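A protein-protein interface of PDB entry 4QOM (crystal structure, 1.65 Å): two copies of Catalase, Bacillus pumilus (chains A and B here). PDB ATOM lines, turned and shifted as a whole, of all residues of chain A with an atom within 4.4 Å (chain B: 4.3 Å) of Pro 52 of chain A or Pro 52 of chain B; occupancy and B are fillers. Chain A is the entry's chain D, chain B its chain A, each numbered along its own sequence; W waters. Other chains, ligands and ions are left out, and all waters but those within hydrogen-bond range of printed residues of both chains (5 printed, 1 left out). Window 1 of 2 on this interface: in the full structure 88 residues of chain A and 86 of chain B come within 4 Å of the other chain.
Of the 7 printed residues of chain A, 5 touch a printed residue of chain B. Printed residues of chain A that touch a printed residue of chain B: Arg 50, Ile 51, Pro 52, Glu 53 and His 346. Hydrophobic or aromatic side chains of chain A within 4 Å of the printed part of chain B: Pro 52 and His 346. Of the 7 printed residues of chain B, 4 touch a printed residue of chain A. Printed residues of chain B that touch a printed residue of chain A: Arg 50, Pro 52, Glu 53 and His 346. Among the printed residues, 8 pairs touch across the chains. Among the printed residues, no Asp or Glu carboxylate lies within 4 Å of a Lys or Arg side-chain nitrogen of the other chain.
Arg 50 of chain A touches Pro 52 of chain B, and with the chains exchanged Pro 52 of chain A touches Arg 50 of chain B. Arg 50 of chain A touches Glu 53 of chain B, and with the chains exchanged Glu 53 of chain A touches Arg 50 of chain B. Arg 50 of chain A touches His 346 of chain B, and with the chains exchanged His 346 of chain A touches Arg 50 of chain B. Pro 52 of chain A touches its own counterpart, Pro 52 of chain B. Of the 8 pairs that touch across the chains among the printed residues, 7 have their exchanged pair printed and touching as well.
Of chain B, only Arg 50 (3.6 Å) and Pro 52 (3.97 Å) come within 4 Å of Pro 52 of chain A. Of chain A, only Arg 50 (3.6 Å), Ile 51 (3.9 Å) and Pro 52 (3.97 Å) come within 4 Å of Pro 52 of chain B. Printed residues of chain A within 4 Å of Arg 50 of chain B: Pro 52 (3.6 Å), Glu 53 (3.7 Å) and His 346 (3.1 Å). Printed residues of chain B within 4 Å of Glu 53 of chain A: Arg 50 (3.7 Å). Arg 54 of chain A touches none of the printed residues of chain B. Arg 54 of chain B touches none of the printed residues of chain A. The nearest residue of chain B that does not touch Pro 52 of chain A is Ile 51 of chain B (4.02 Å).
A ring nitrogen (NE2) of His 346 of chain A sits at hydrogen-bond distance from the backbone carbonyl oxygen of Arg 50 of chain B (3.1 Å). The backbone carbonyl oxygen (O) of Arg 50 of chain A lies within hydrogen-bond range of a ring nitrogen (NE2) of His 346 of chain B, at 3.0 Å.
Water W2 lies within hydrogen-bond range of the side-chain carboxylate of Glu 53 of chain A (2.6 Å), the backbone carbonyl oxygen of Arg 54 of chain A (2.6 Å) and the guanidinium group of Arg 50 of chain B (3.0 Å). Water W4 bridges OE1 of Glu 53 of chain B (2.7 Å) and OE1 of Glu 53 of chain A (2.7 Å). Water W1 lies within hydrogen-bond range of OE2 of Glu 53 of chain B, O of Arg 54 of chain B and NE of Arg 50 of chain A. Water W3 lies within hydrogen-bond range of O of Ile 51 of chain A (2.7 Å) and N of Glu 53 of chain B (3.0 Å). Water W5 bridges O of Ile 51 of chain B and N of Glu 53 of chain A.
O of Arg 50 of chain A touches CB of Pro 52 of chain B (3.6 Å). Arg 50 of chain A touches Glu 53 of chain B. Ile 51 of chain A touches Pro 52 of chain B. O of Arg 50 of chain B touches CB of Pro 52 of chain A, at 3.6 Å. Pro 52 of chain A touches Pro 52 of chain B. Glu 53 of chain A touches Arg 50 of chain B (O to CB, 3.7 Å).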
ATOM      1  N   ARG A  50      25.606  -1.012  13.252  1.00  0.00           N
ATOM      2  CA  ARG A  50      26.209  -1.359  11.977  1.00  0.00           C
ATOM      3  C   ARG A  50      25.835  -2.744  11.557  1.00  0.00           C
ATOM      4  O   ARG A  50      25.800  -3.723  12.328  1.00  0.00           O
ATOM      5  CB  ARG A  50      27.724  -1.192  12.034  1.00  0.00           C
ATOM      6  CG  ARG A  50      28.209   0.172  12.467  1.00  0.00           C
ATOM      7  CD  ARG A  50      27.926   1.315  11.460  1.00  0.00           C
ATOM      8  NE  ARG A  50      28.372   2.537  12.132  1.00  0.00           N
ATOM      9  CZ  ARG A  50      27.607   3.404  12.754  1.00  0.00           C
ATOM     10  NH1 ARG A  50      26.308   3.274  12.824  1.00  0.00           N
ATOM     11  NH2 ARG A  50      28.222   4.354  13.499  1.00  0.00           N
ATOM     12  N   ILE A  51      25.617  -2.866  10.230  1.00  0.00           N
ATOM     13  CA  ILE A  51      25.492  -4.136   9.510  1.00  0.00           C
ATOM     14  C   ILE A  51      26.629  -4.256   8.528  1.00  0.00           C
ATOM     15  O   ILE A  51      27.249  -3.250   8.139  1.00  0.00           O
ATOM     16  CB  ILE A  51      24.082  -4.261   8.904  1.00  0.00           C
ATOM     17  CG1 ILE A  51      23.858  -3.290   7.732  1.00  0.00           C
ATOM     18  CG2 ILE A  51      23.039  -3.968  10.029  1.00  0.00           C
ATOM     19  CD1 ILE A  51      22.573  -3.459   7.003  1.00  0.00           C
ATOM     20  N   PRO A  52      26.844  -5.460   7.949  1.00  0.00           N
ATOM     21  CA  PRO A  52      27.893  -5.560   6.884  1.00  0.00           C
ATOM     22  C   PRO A  52      27.595  -4.669   5.724  1.00  0.00           C
ATOM     23  O   PRO A  52      26.434  -4.525   5.334  1.00  0.00           O
ATOM     24  CB  PRO A  52      27.871  -7.027   6.516  1.00  0.00           C
ATOM     25  CG  PRO A  52      27.187  -7.724   7.654  1.00  0.00           C
ATOM     26  CD  PRO A  52      26.160  -6.739   8.146  1.00  0.00           C
ATOM     27  N   GLU A  53      28.630  -4.035   5.169  1.00  0.00           N
ATOM     28  CA  GLU A  53      28.496  -3.301   3.879  1.00  0.00           C
ATOM     29  C   GLU A  53      28.391  -4.297   2.753  1.00  0.00           C
ATOM     30  O   GLU A  53      28.745  -5.482   2.894  1.00  0.00           O
ATOM     31  CB  GLU A  53      29.644  -2.320   3.612  1.00  0.00           C
ATOM     32  CG  GLU A  53      30.959  -2.926   3.206  1.00  0.00           C
ATOM     33  CD  GLU A  53      32.100  -1.928   3.054  1.00  0.00           C
ATOM     34  OE1 GLU A  53      32.057  -0.779   3.671  1.00  0.00           O
ATOM     35  OE2 GLU A  53      33.090  -2.348   2.376  1.00  0.00           O
ATOM     36  N   ARG A  54      27.906  -3.800   1.659  1.00  0.00           N
ATOM     37  CA  ARG A  54      27.878  -4.599   0.430  1.00  0.00           C
ATOM     38  C   ARG A  54      29.284  -5.107   0.081  1.00  0.00           C
ATOM     39  O   ARG A  54      30.255  -4.382   0.183  1.00  0.00           O
ATOM     40  CB  ARG A  54      27.276  -3.810  -0.740  1.00  0.00           C
ATOM     41  CG  ARG A  54      25.815  -3.419  -0.670  1.00  0.00           C
ATOM     42  CD  ARG A  54      25.530  -2.289  -1.620  1.00  0.00           C
ATOM     43  NE  ARG A  54      24.097  -1.932  -1.583  1.00  0.00           N
ATOM     44  CZ  ARG A  54      23.499  -1.247  -0.601  1.00  0.00           C
ATOM     45  NH1 ARG A  54      24.153  -0.857   0.473  1.00  0.00           N
ATOM     46  NH2 ARG A  54      22.192  -0.984  -0.676  1.00  0.00           N
ATOM     47  N   HIS A 346      22.299 -12.693   4.068  1.00  0.00           N
ATOM     48  CA  HIS A 346      23.380 -12.467   5.002  1.00  0.00           C
ATOM     49  C   HIS A 346      23.452 -11.032   5.483  1.00  0.00           C
ATOM     50  O   HIS A 346      23.551 -10.784   6.733  1.00  0.00           O
ATOM     51  CB  HIS A 346      24.700 -12.896   4.372  1.00  0.00           C
ATOM     52  CG  HIS A 346      25.921 -12.313   5.028  1.00  0.00           C
ATOM     53  ND1 HIS A 346      26.411 -12.788   6.204  1.00  0.00           N
ATOM     54  CD2 HIS A 346      26.808 -11.398   4.584  1.00  0.00           C
ATOM     55  CE1 HIS A 346      27.491 -12.112   6.533  1.00  0.00           C
ATOM     56  NE2 HIS A 346      27.750 -11.245   5.570  1.00  0.00           N
ATOM     57  N   ARG A 347      23.477 -10.085   4.541  1.00  0.00           N
ATOM     58  CA  ARG A 347      23.730  -8.672   4.822  1.00  0.00           C
ATOM     59  C   ARG A 347      22.553  -8.019   5.574  1.00  0.00           C
ATOM     60  O   ARG A 347      22.764  -7.195   6.474  1.00  0.00           O
ATOM     61  CB  ARG A 347      24.019  -7.923   3.533  1.00  0.00           C
ATOM     62  CG  ARG A 347      24.300  -6.452   3.719  1.00  0.00           C
ATOM     63  CD  ARG A 347      24.752  -5.809   2.424  1.00  0.00           C
ATOM     64  NE  ARG A 347      23.779  -5.680   1.355  1.00  0.00           N
ATOM     65  CZ  ARG A 347      22.880  -4.683   1.180  1.00  0.00           C
ATOM     66  NH1 ARG A 347      22.736  -3.733   2.122  1.00  0.00           N
ATOM     67  NH2 ARG A 347      22.045  -4.705   0.134  1.00  0.00           N
ATOM     68  N   ARG B  50      31.942 -10.054   4.319  1.00  0.00           N
ATOM     69  CA  ARG B  50      31.957  -8.867   5.077  1.00  0.00           C
ATOM     70  C   ARG B  50      31.265  -9.039   6.422  1.00  0.00           C
ATOM     71  O   ARG B  50      30.231  -9.698   6.535  1.00  0.00           O
ATOM     72  CB  ARG B  50      31.289  -7.725   4.284  1.00  0.00           C
ATOM     73  CG  ARG B  50      31.953  -7.378   2.986  1.00  0.00           C
ATOM     74  CD  ARG B  50      33.383  -6.810   3.057  1.00  0.00           C
ATOM     75  NE  ARG B  50      33.817  -6.687   1.669  1.00  0.00           N
ATOM     76  CZ  ARG B  50      34.555  -7.553   1.003  1.00  0.00           C
ATOM     77  NH1 ARG B  50      35.132  -8.591   1.616  1.00  0.00           N
ATOM     78  NH2 ARG B  50      34.697  -7.379  -0.274  1.00  0.00           N
ATOM     79  N   ILE B  51      31.847  -8.375   7.409  1.00  0.00           N
ATOM     80  CA  ILE B  51      31.268  -8.286   8.770  1.00  0.00           C
ATOM     81  C   ILE B  51      31.029  -6.789   9.084  1.00  0.00           C
ATOM     82  O   ILE B  51      31.641  -5.896   8.439  1.00  0.00           O
ATOM     83  CB  ILE B  51      32.113  -9.020   9.834  1.00  0.00           C
ATOM     84  CG1 ILE B  51      33.427  -8.306  10.057  1.00  0.00           C
ATOM     85  CG2 ILE B  51      32.332 -10.448   9.301  1.00  0.00           C
ATOM     86  CD1 ILE B  51      34.252  -8.846  11.196  1.00  0.00           C
ATOM     87  N   PRO B  52      30.146  -6.512  10.010  1.00  0.00           N
ATOM     88  CA  PRO B  52      30.006  -5.063  10.362  1.00  0.00           C
ATOM     89  C   PRO B  52      31.307  -4.377  10.762  1.00  0.00           C
ATOM     90  O   PRO B  52      32.158  -4.988  11.339  1.00  0.00           O
ATOM     91  CB  PRO B  52      29.058  -5.103  11.573  1.00  0.00           C
ATOM     92  CG  PRO B  52      28.381  -6.412  11.548  1.00  0.00           C
ATOM     93  CD  PRO B  52      29.431  -7.359  10.967  1.00  0.00           C
ATOM     94  N   GLU B  53      31.473  -3.114  10.349  1.00  0.00           N
ATOM     95  CA  GLU B  53      32.640  -2.352  10.676  1.00  0.00           C
ATOM     96  C   GLU B  53      32.429  -1.874  12.086  1.00  0.00           C
ATOM     97  O   GLU B  53      31.302  -1.852  12.635  1.00  0.00           O
ATOM     98  CB  GLU B  53      32.945  -1.144   9.756  1.00  0.00           C
ATOM     99  CG  GLU B  53      31.974  -0.025   9.854  1.00  0.00           C
ATOM    100  CD  GLU B  53      32.267   1.129   8.883  1.00  0.00           C
ATOM    101  OE1 GLU B  53      32.913   0.920   7.786  1.00  0.00           O
ATOM    102  OE2 GLU B  53      31.770   2.241   9.187  1.00  0.00           O
ATOM    103  N   ARG B  54      33.512  -1.436  12.666  1.00  0.00           N
ATOM    104  CA  ARG B  54      33.388  -0.880  14.038  1.00  0.00           C
ATOM    105  C   ARG B  54      32.471   0.342  14.030  1.00  0.00           C
ATOM    106  O   ARG B  54      32.522   1.159  13.105  1.00  0.00           O
ATOM    107  CB  ARG B  54      34.764  -0.446  14.577  1.00  0.00           C
ATOM    108  CG  ARG B  54      35.768  -1.558  14.848  1.00  0.00           C
ATOM    109  CD  ARG B  54      37.185  -0.984  14.908  1.00  0.00           C
ATOM    110  NE  ARG B  54      38.167  -2.032  15.234  1.00  0.00           N
ATOM    111  CZ  ARG B  54      38.604  -2.971  14.423  1.00  0.00           C
ATOM    112  NH1 ARG B  54      38.113  -3.104  13.210  1.00  0.00           N
ATOM    113  NH2 ARG B  54      39.469  -3.883  14.865  1.00  0.00           N
ATOM    114  N   HIS B 346      28.488  -8.718  19.044  1.00  0.00           N
ATOM    115  CA  HIS B 346      27.748  -8.453  17.828  1.00  0.00           C
ATOM    116  C   HIS B 346      28.646  -8.456  16.569  1.00  0.00           C
ATOM    117  O   HIS B 346      28.302  -9.140  15.538  1.00  0.00           O
ATOM    118  CB  HIS B 346      27.026  -7.117  17.966  1.00  0.00           C
ATOM    119  CG  HIS B 346      26.644  -6.475  16.671  1.00  0.00           C
ATOM    120  ND1 HIS B 346      25.616  -6.946  15.890  1.00  0.00           N
ATOM    121  CD2 HIS B 346      27.118  -5.379  16.030  1.00  0.00           C
ATOM    122  CE1 HIS B 346      25.422  -6.144  14.867  1.00  0.00           C
ATOM    123  NE2 HIS B 346      26.360  -5.213  14.893  1.00  0.00           N
ATOM    124  N   ARG B 347      29.735  -7.675  16.612  1.00  0.00           N
ATOM    125  CA  ARG B 347      30.569  -7.457  15.411  1.00  0.00           C
ATOM    126  C   ARG B 347      31.298  -8.738  14.978  1.00  0.00           C
ATOM    127  O   ARG B 347      31.483  -9.019  13.795  1.00  0.00           O
ATOM    128  CB  ARG B 347      31.541  -6.309  15.704  1.00  0.00           C
ATOM    129  CG  ARG B 347      32.453  -5.946  14.540  1.00  0.00           C
ATOM    130  CD  ARG B 347      33.259  -4.688  14.785  1.00  0.00           C
ATOM    131  NE  ARG B 347      34.277  -4.715  15.832  1.00  0.00           N
ATOM    132  CZ  ARG B 347      35.529  -5.166  15.679  1.00  0.00           C
ATOM    133  NH1 ARG B 347      35.925  -5.681  14.500  1.00  0.00           N
ATOM    134  NH2 ARG B 347      36.427  -5.081  16.681  1.00  0.00           N
HETATM  135  O   HOH W   1      31.196   3.108  11.648  1.00  0.00           O
HETATM  136  O   HOH W   2      32.861  -4.134   0.491  1.00  0.00           O
HETATM  137  O   HOH W   3      29.657  -2.001   8.203  1.00  0.00           O
HETATM  138  O   HOH W   4      31.731  -0.974   6.354  1.00  0.00           O
HETATM  139  O   HOH W   5      31.325  -4.102   6.298  1.00  0.00           O
